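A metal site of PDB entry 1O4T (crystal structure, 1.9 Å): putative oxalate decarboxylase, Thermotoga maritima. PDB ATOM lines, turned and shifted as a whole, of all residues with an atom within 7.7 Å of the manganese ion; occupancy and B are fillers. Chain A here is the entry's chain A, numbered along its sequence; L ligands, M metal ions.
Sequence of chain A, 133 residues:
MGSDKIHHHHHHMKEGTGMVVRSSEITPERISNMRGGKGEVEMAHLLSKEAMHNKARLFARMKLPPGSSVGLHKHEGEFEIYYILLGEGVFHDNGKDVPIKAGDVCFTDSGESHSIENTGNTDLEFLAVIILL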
ATOM      1  N   MET A  34     -22.110  17.158  15.297  1.00  0.00           N
ATOM      2  CA  MET A  34     -21.983  17.235  16.724  1.00  0.00           C
ATOM      3  C   MET A  34     -20.887  16.262  17.160  1.00  0.00           C
ATOM      4  O   MET A  34     -20.941  15.085  16.817  1.00  0.00           O
ATOM      5  CB  MET A  34     -23.288  16.856  17.410  1.00  0.00           C
ATOM      6  CG  MET A  34     -23.234  17.092  18.910  1.00  0.00           C
ATOM      7  SD  MET A  34     -24.699  16.660  19.728  1.00  0.00           S
ATOM      8  CE  MET A  34     -24.227  17.316  21.257  1.00  0.00           C
ATOM      9  N   ARG A  35     -19.925  16.778  17.908  1.00  0.00           N
ATOM     10  CA  ARG A  35     -18.729  16.038  18.290  1.00  0.00           C
ATOM     11  C   ARG A  35     -18.053  15.359  17.127  1.00  0.00           C
ATOM     12  O   ARG A  35     -17.511  14.271  17.267  1.00  0.00           O
ATOM     13  CB  ARG A  35     -19.059  15.025  19.375  1.00  0.00           C
ATOM     14  CG  ARG A  35     -19.760  15.614  20.610  1.00  0.00           C
ATOM     15  CD  ARG A  35     -19.259  16.985  21.013  1.00  0.00           C
ATOM     16  NE  ARG A  35     -18.136  16.887  21.932  1.00  0.00           N
ATOM     17  CZ  ARG A  35     -18.234  17.021  23.257  1.00  0.00           C
ATOM     18  NH1 ARG A  35     -17.131  16.895  23.997  1.00  0.00           N
ATOM     19  NH2 ARG A  35     -19.411  17.260  23.847  1.00  0.00           N
ATOM     20  N   ARG A  57     -24.696  18.153  34.544  1.00  0.00           N
ATOM     21  CA  ARG A  57     -24.460  19.288  33.683  1.00  0.00           C
ATOM     22  C   ARG A  57     -25.307  19.274  32.393  1.00  0.00           C
ATOM     23  O   ARG A  57     -25.315  20.284  31.677  1.00  0.00           O
ATOM     24  CB  ARG A  57     -22.954  19.454  33.390  1.00  0.00           C
ATOM     25  CG  ARG A  57     -22.369  18.571  32.287  1.00  0.00           C
ATOM     26  CD  ARG A  57     -20.935  19.005  31.898  1.00  0.00           C
ATOM     27  NE  ARG A  57     -20.292  18.119  30.925  1.00  0.00           N
ATOM     28  CZ  ARG A  57     -20.570  18.097  29.624  1.00  0.00           C
ATOM     29  NH1 ARG A  57     -21.454  18.920  29.083  1.00  0.00           N
ATOM     30  NH2 ARG A  57     -19.933  17.248  28.847  1.00  0.00           N
ATOM     31  N   LEU A  58     -25.992  18.157  32.116  1.00  0.00           N
ATOM     32  CA  LEU A  58     -26.855  18.019  30.949  1.00  0.00           C
ATOM     33  C   LEU A  58     -28.070  17.142  31.252  1.00  0.00           C
ATOM     34  O   LEU A  58     -27.922  16.053  31.783  1.00  0.00           O
ATOM     35  CB  LEU A  58     -26.101  17.349  29.787  1.00  0.00           C
ATOM     36  CG  LEU A  58     -26.869  17.279  28.450  1.00  0.00           C
ATOM     37  CD1 LEU A  58     -27.020  18.680  27.866  1.00  0.00           C
ATOM     38  CD2 LEU A  58     -26.153  16.375  27.492  1.00  0.00           C
ATOM     39  N   VAL A  70     -23.996  11.406  16.597  1.00  0.00           N
ATOM     40  CA  VAL A  70     -23.124  12.168  17.491  1.00  0.00           C
ATOM     41  C   VAL A  70     -21.779  11.468  17.445  1.00  0.00           C
ATOM     42  O   VAL A  70     -21.703  10.258  17.618  1.00  0.00           O
ATOM     43  CB  VAL A  70     -23.617  12.155  18.926  1.00  0.00           C
ATOM     44  CG1 VAL A  70     -22.680  12.920  19.805  1.00  0.00           C
ATOM     45  CG2 VAL A  70     -25.032  12.722  19.004  1.00  0.00           C
ATOM     46  N   GLY A  71     -20.717  12.232  17.214  1.00  0.00           N
ATOM     47  CA  GLY A  71     -19.405  11.694  16.943  1.00  0.00           C
ATOM     48  C   GLY A  71     -18.725  11.198  18.190  1.00  0.00           C
ATOM     49  O   GLY A  71     -19.164  11.474  19.291  1.00  0.00           O
ATOM     50  N   LEU A  72     -17.669  10.421  17.999  1.00  0.00           N
ATOM     51  CA  LEU A  72     -16.931   9.843  19.111  1.00  0.00           C
ATOM     52  C   LEU A  72     -16.329  10.954  19.964  1.00  0.00           C
ATOM     53  O   LEU A  72     -15.687  11.868  19.446  1.00  0.00           O
ATOM     54  CB  LEU A  72     -15.845   8.859  18.624  1.00  0.00           C
ATOM     55  CG  LEU A  72     -15.022   8.049  19.642  1.00  0.00           C
ATOM     56  CD1 LEU A  72     -15.879   6.971  20.289  1.00  0.00           C
ATOM     57  CD2 LEU A  72     -13.801   7.417  18.996  1.00  0.00           C
ATOM     58  N   HIS A  73     -16.590  10.895  21.283  1.00  0.00           N
ATOM     59  CA  HIS A  73     -15.972  11.812  22.222  1.00  0.00           C
ATOM     60  C   HIS A  73     -15.890  11.149  23.575  1.00  0.00           C
ATOM     61  O   HIS A  73     -16.621  10.207  23.869  1.00  0.00           O
ATOM     62  CB  HIS A  73     -16.777  13.097  22.363  1.00  0.00           C
ATOM     63  CG  HIS A  73     -18.169  12.851  22.828  1.00  0.00           C
ATOM     64  ND1 HIS A  73     -19.110  12.236  22.037  1.00  0.00           N
ATOM     65  CD2 HIS A  73     -18.760  13.069  24.030  1.00  0.00           C
ATOM     66  CE1 HIS A  73     -20.229  12.109  22.720  1.00  0.00           C
ATOM     67  NE2 HIS A  73     -20.055  12.621  23.923  1.00  0.00           N
ATOM     68  N   LYS A  74     -15.016  11.703  24.385  1.00  0.00           N
ATOM     69  CA  LYS A  74     -14.635  11.175  25.683  1.00  0.00           C
ATOM     70  C   LYS A  74     -15.277  11.979  26.802  1.00  0.00           C
ATOM     71  O   LYS A  74     -15.433  13.196  26.699  1.00  0.00           O
ATOM     72  CB  LYS A  74     -13.116  11.286  25.821  1.00  0.00           C
ATOM     73  CG  LYS A  74     -12.571  10.680  27.083  1.00  0.00           C
ATOM     74  CD  LYS A  74     -11.089  10.718  27.048  1.00  0.00           C
ATOM     75  CE  LYS A  74     -10.484  10.133  28.315  1.00  0.00           C
ATOM     76  NZ  LYS A  74      -9.024  10.279  28.209  1.00  0.00           N
ATOM     77  N   HIS A  75     -15.613  11.284  27.886  1.00  0.00           N
ATOM     78  CA  HIS A  75     -16.086  11.872  29.128  1.00  0.00           C
ATOM     79  C   HIS A  75     -15.076  11.625  30.245  1.00  0.00           C
ATOM     80  O   HIS A  75     -14.612  10.515  30.404  1.00  0.00           O
ATOM     81  CB  HIS A  75     -17.471  11.300  29.449  1.00  0.00           C
ATOM     82  CG  HIS A  75     -18.553  11.831  28.545  1.00  0.00           C
ATOM     83  ND1 HIS A  75     -19.106  13.067  28.731  1.00  0.00           N
ATOM     84  CD2 HIS A  75     -19.107  11.333  27.410  1.00  0.00           C
ATOM     85  CE1 HIS A  75     -19.981  13.315  27.777  1.00  0.00           C
ATOM     86  NE2 HIS A  75     -20.026  12.265  26.975  1.00  0.00           N
ATOM     87  N   GLU A  78     -17.011  12.651  34.822  1.00  0.00           N
ATOM     88  CA  GLU A  78     -18.467  12.603  34.748  1.00  0.00           C
ATOM     89  C   GLU A  78     -18.878  11.305  34.084  1.00  0.00           C
ATOM     90  O   GLU A  78     -18.025  10.573  33.570  1.00  0.00           O
ATOM     91  CB  GLU A  78     -19.017  13.794  33.938  1.00  0.00           C
ATOM     92  CG  GLU A  78     -18.581  13.777  32.487  1.00  0.00           C
ATOM     93  CD  GLU A  78     -18.670  15.120  31.788  1.00  0.00           C
ATOM     94  OE1 GLU A  78     -18.911  16.138  32.464  1.00  0.00           O
ATOM     95  OE2 GLU A  78     -18.485  15.118  30.540  1.00  0.00           O
ATOM     96  N   PHE A  79     -20.174  11.007  34.075  1.00  0.00           N
ATOM     97  CA  PHE A  79     -20.682   9.882  33.324  1.00  0.00           C
ATOM     98  C   PHE A  79     -21.966  10.260  32.628  1.00  0.00           C
ATOM     99  O   PHE A  79     -22.628  11.210  33.036  1.00  0.00           O
ATOM    100  CB  PHE A  79     -20.807   8.623  34.206  1.00  0.00           C
ATOM    101  CG  PHE A  79     -21.812   8.737  35.315  1.00  0.00           C
ATOM    102  CD1 PHE A  79     -21.429   9.153  36.565  1.00  0.00           C
ATOM    103  CD2 PHE A  79     -23.144   8.391  35.110  1.00  0.00           C
ATOM    104  CE1 PHE A  79     -22.330   9.252  37.588  1.00  0.00           C
ATOM    105  CE2 PHE A  79     -24.079   8.516  36.151  1.00  0.00           C
ATOM    106  CZ  PHE A  79     -23.639   8.939  37.408  1.00  0.00           C
ATOM    107  N   GLU A  80     -22.282   9.557  31.547  1.00  0.00           N
ATOM    108  CA  GLU A  80     -23.489   9.824  30.765  1.00  0.00           C
ATOM    109  C   GLU A  80     -24.380   8.610  30.572  1.00  0.00           C
ATOM    110  O   GLU A  80     -23.898   7.509  30.366  1.00  0.00           O
ATOM    111  CB  GLU A  80     -23.108  10.389  29.387  1.00  0.00           C
ATOM    112  CG  GLU A  80     -24.234  11.189  28.770  1.00  0.00           C
ATOM    113  CD  GLU A  80     -23.814  11.998  27.579  1.00  0.00           C
ATOM    114  OE1 GLU A  80     -24.674  12.668  26.976  1.00  0.00           O
ATOM    115  OE2 GLU A  80     -22.633  11.967  27.237  1.00  0.00           O
ATOM    116  N   ILE A  81     -25.672   8.856  30.643  1.00  0.00           N
ATOM    117  CA  ILE A  81     -26.690   7.862  30.400  1.00  0.00           C
ATOM    118  C   ILE A  81     -27.529   8.335  29.213  1.00  0.00           C
ATOM    119  O   ILE A  81     -27.984   9.462  29.174  1.00  0.00           O
ATOM    120  CB  ILE A  81     -27.615   7.733  31.643  1.00  0.00           C
ATOM    121  CG1 ILE A  81     -26.805   7.477  32.921  1.00  0.00           C
ATOM    122  CG2 ILE A  81     -28.697   6.647  31.408  1.00  0.00           C
ATOM    123  CD1 ILE A  81     -27.600   7.842  34.166  1.00  0.00           C
ATOM    124  N   TYR A  82     -27.726   7.470  28.234  1.00  0.00           N
ATOM    125  CA  TYR A  82     -28.789   7.673  27.275  1.00  0.00           C
ATOM    126  C   TYR A  82     -29.970   6.744  27.593  1.00  0.00           C
ATOM    127  O   TYR A  82     -29.775   5.553  27.901  1.00  0.00           O
ATOM    128  CB  TYR A  82     -28.316   7.305  25.881  1.00  0.00           C
ATOM    129  CG  TYR A  82     -27.164   8.076  25.237  1.00  0.00           C
ATOM    130  CD1 TYR A  82     -26.485   7.529  24.151  1.00  0.00           C
ATOM    131  CD2 TYR A  82     -26.788   9.351  25.674  1.00  0.00           C
ATOM    132  CE1 TYR A  82     -25.497   8.220  23.518  1.00  0.00           C
ATOM    133  CE2 TYR A  82     -25.801  10.042  25.042  1.00  0.00           C
ATOM    134  CZ  TYR A  82     -25.134   9.478  23.959  1.00  0.00           C
ATOM    135  OH  TYR A  82     -24.110  10.198  23.348  1.00  0.00           O
ATOM    136  N   PHE A  91     -25.051   2.226  19.181  1.00  0.00           N
ATOM    137  CA  PHE A  91     -24.300   2.861  20.242  1.00  0.00           C
ATOM    138  C   PHE A  91     -22.891   2.279  20.290  1.00  0.00           C
ATOM    139  O   PHE A  91     -22.699   1.048  20.272  1.00  0.00           O
ATOM    140  CB  PHE A  91     -25.007   2.548  21.555  1.00  0.00           C
ATOM    141  CG  PHE A  91     -24.337   3.102  22.762  1.00  0.00           C
ATOM    142  CD1 PHE A  91     -24.220   4.466  22.939  1.00  0.00           C
ATOM    143  CD2 PHE A  91     -23.854   2.270  23.739  1.00  0.00           C
ATOM    144  CE1 PHE A  91     -23.625   5.010  24.062  1.00  0.00           C
ATOM    145  CE2 PHE A  91     -23.235   2.835  24.907  1.00  0.00           C
ATOM    146  CZ  PHE A  91     -23.131   4.196  25.035  1.00  0.00           C
ATOM    147  N   THR A 108     -22.333   5.332  29.780  1.00  0.00           N
ATOM    148  CA  THR A 108     -20.911   5.611  29.502  1.00  0.00           C
ATOM    149  C   THR A 108     -20.235   6.153  30.750  1.00  0.00           C
ATOM    150  O   THR A 108     -20.646   7.159  31.292  1.00  0.00           O
ATOM    151  CB  THR A 108     -20.770   6.604  28.371  1.00  0.00           C
ATOM    152  OG1 THR A 108     -21.284   6.031  27.178  1.00  0.00           O
ATOM    153  CG2 THR A 108     -19.324   6.833  28.028  1.00  0.00           C
ATOM    154  N   GLU A 112     -14.377   6.683  29.551  1.00  0.00           N
ATOM    155  CA  GLU A 112     -14.773   6.078  28.290  1.00  0.00           C
ATOM    156  C   GLU A 112     -15.185   7.104  27.238  1.00  0.00           C
ATOM    157  O   GLU A 112     -15.610   8.193  27.543  1.00  0.00           O
ATOM    158  CB  GLU A 112     -15.944   5.120  28.493  1.00  0.00           C
ATOM    159  CG  GLU A 112     -15.731   4.085  29.573  1.00  0.00           C
ATOM    160  CD  GLU A 112     -16.819   3.018  29.586  1.00  0.00           C
ATOM    161  OE1 GLU A 112     -18.047   3.320  29.434  1.00  0.00           O
ATOM    162  OE2 GLU A 112     -16.437   1.860  29.777  1.00  0.00           O
ATOM    163  N   SER A 113     -15.106   6.702  25.979  1.00  0.00           N
ATOM    164  CA  SER A 113     -15.552   7.510  24.861  1.00  0.00           C
ATOM    165  C   SER A 113     -16.728   6.798  24.222  1.00  0.00           C
ATOM    166  O   SER A 113     -16.776   5.559  24.220  1.00  0.00           O
ATOM    167  CB  SER A 113     -14.448   7.672  23.830  1.00  0.00           C
ATOM    168  OG  SER A 113     -13.293   8.265  24.397  1.00  0.00           O
ATOM    169  N   HIS A 114     -17.671   7.578  23.676  1.00  0.00           N
ATOM    170  CA  HIS A 114     -18.827   7.018  22.995  1.00  0.00           C
ATOM    171  C   HIS A 114     -19.295   7.844  21.789  1.00  0.00           C
ATOM    172  O   HIS A 114     -18.822   8.982  21.570  1.00  0.00           O
ATOM    173  CB  HIS A 114     -20.026   6.773  23.979  1.00  0.00           C
ATOM    174  CG  HIS A 114     -20.676   8.027  24.507  1.00  0.00           C
ATOM    175  ND1 HIS A 114     -21.737   7.971  25.390  1.00  0.00           N
ATOM    176  CD2 HIS A 114     -20.379   9.337  24.355  1.00  0.00           C
ATOM    177  CE1 HIS A 114     -22.080   9.204  25.742  1.00  0.00           C
ATOM    178  NE2 HIS A 114     -21.273  10.057  25.136  1.00  0.00           N
ATOM    179  N   SER A 115     -20.218   7.235  21.034  1.00  0.00           N
ATOM    180  CA  SER A 115     -20.858   7.848  19.877  1.00  0.00           C
ATOM    181  C   SER A 115     -22.175   7.155  19.693  1.00  0.00           C
ATOM    182  O   SER A 115     -22.395   6.098  20.291  1.00  0.00           O
ATOM    183  CB  SER A 115     -20.024   7.690  18.605  1.00  0.00           C
ATOM    184  OG  SER A 115     -19.864   6.345  18.259  1.00  0.00           O
ATOM    185  N   ALA A 128     -30.494  12.325  27.233  1.00  0.00           N
ATOM    186  CA  ALA A 128     -29.073  12.313  27.625  1.00  0.00           C
ATOM    187  C   ALA A 128     -28.907  13.051  28.935  1.00  0.00           C
ATOM    188  O   ALA A 128     -29.342  14.197  29.056  1.00  0.00           O
ATOM    189  CB  ALA A 128     -28.237  12.927  26.559  1.00  0.00           C
ATOM    190  N   VAL A 129     -28.242  12.412  29.903  1.00  0.00           N
ATOM    191  CA  VAL A 129     -28.039  12.999  31.200  1.00  0.00           C
ATOM    192  C   VAL A 129     -26.551  12.842  31.582  1.00  0.00           C
ATOM    193  O   VAL A 129     -26.043  11.744  31.617  1.00  0.00           O
ATOM    194  CB  VAL A 129     -28.883  12.287  32.293  1.00  0.00           C
ATOM    195  CG1 VAL A 129     -28.919  13.126  33.544  1.00  0.00           C
ATOM    196  CG2 VAL A 129     -30.278  12.061  31.790  1.00  0.00           C
ATOM    197  N   ILE A 130     -25.866  13.933  31.891  1.00  0.00           N
ATOM    198  CA  ILE A 130     -24.472  13.838  32.272  1.00  0.00           C
ATOM    199  C   ILE A 130     -24.389  14.160  33.752  1.00  0.00           C
ATOM    200  O   ILE A 130     -24.837  15.206  34.147  1.00  0.00           O
ATOM    201  CB  ILE A 130     -23.611  14.800  31.433  1.00  0.00           C
ATOM    202  CG1 ILE A 130     -23.718  14.441  29.961  1.00  0.00           C
ATOM    203  CG2 ILE A 130     -22.145  14.738  31.889  1.00  0.00           C
ATOM    204  CD1 ILE A 130     -23.037  15.475  28.997  1.00  0.00           C
HETATM  205  C1  LIG L   1     -23.523  13.587  24.341  1.00  0.00           C
HETATM  206  C2  LIG L   1     -22.750  14.664  24.959  1.00  0.00           C
HETATM  207  O1  LIG L   1     -24.730  13.943  23.843  1.00  0.00           O
HETATM  208  O2  LIG L   1     -23.208  15.917  24.772  1.00  0.00           O
HETATM  209  O3  LIG L   1     -23.109  12.410  24.299  1.00  0.00           O
HETATM  210  O4  LIG L   1     -21.764  14.441  25.669  1.00  0.00           O
HETATM  211 MN    MN M   1     -21.437  12.173  25.525  1.00  0.00          MN
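The side-chain hydroxyl (OH) of Tyr 82 sits close to a ring nitrogen (NE2) of His 114 (3.4 Å).
The backbone NH of His 75 is in hydrogen-bond range of the backbone carbonyl oxygen of Glu 112, 3.1 Å away.
OE2 of Glu 78 sits at hydrogen-bond distance from ND1 of His 75 (2.8 Å).
ND1 of His 114 is in hydrogen-bond range of OG1 of Thr 108 (2.7 Å).
O of Gly 71 sits at hydrogen-bond distance from ND1 of His 73, at 2.9 Å.
O of Glu 80 is in hydrogen-bond range of N of Thr 108.
Residues that only touch the manganese ion: Tyr 82 (3.97 Å).
Of the 24 residues printed, 5 come within 4 Å of the manganese ion.
The nearest printed residue that does not touch the manganese ion is Ile 130 (5.1 Å).
The manganese ion is bound by NE2 of His 75 (2.0 Å), O3 of the ligand (2.1 Å), OE2 of Glu 80 (2.1 Å), NE2 of His 114 (2.2 Å), NE2 of His 73 (2.2 Å) and O4 of the ligand (2.3 Å).
The manganese ion has six donor atoms within binding distance.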
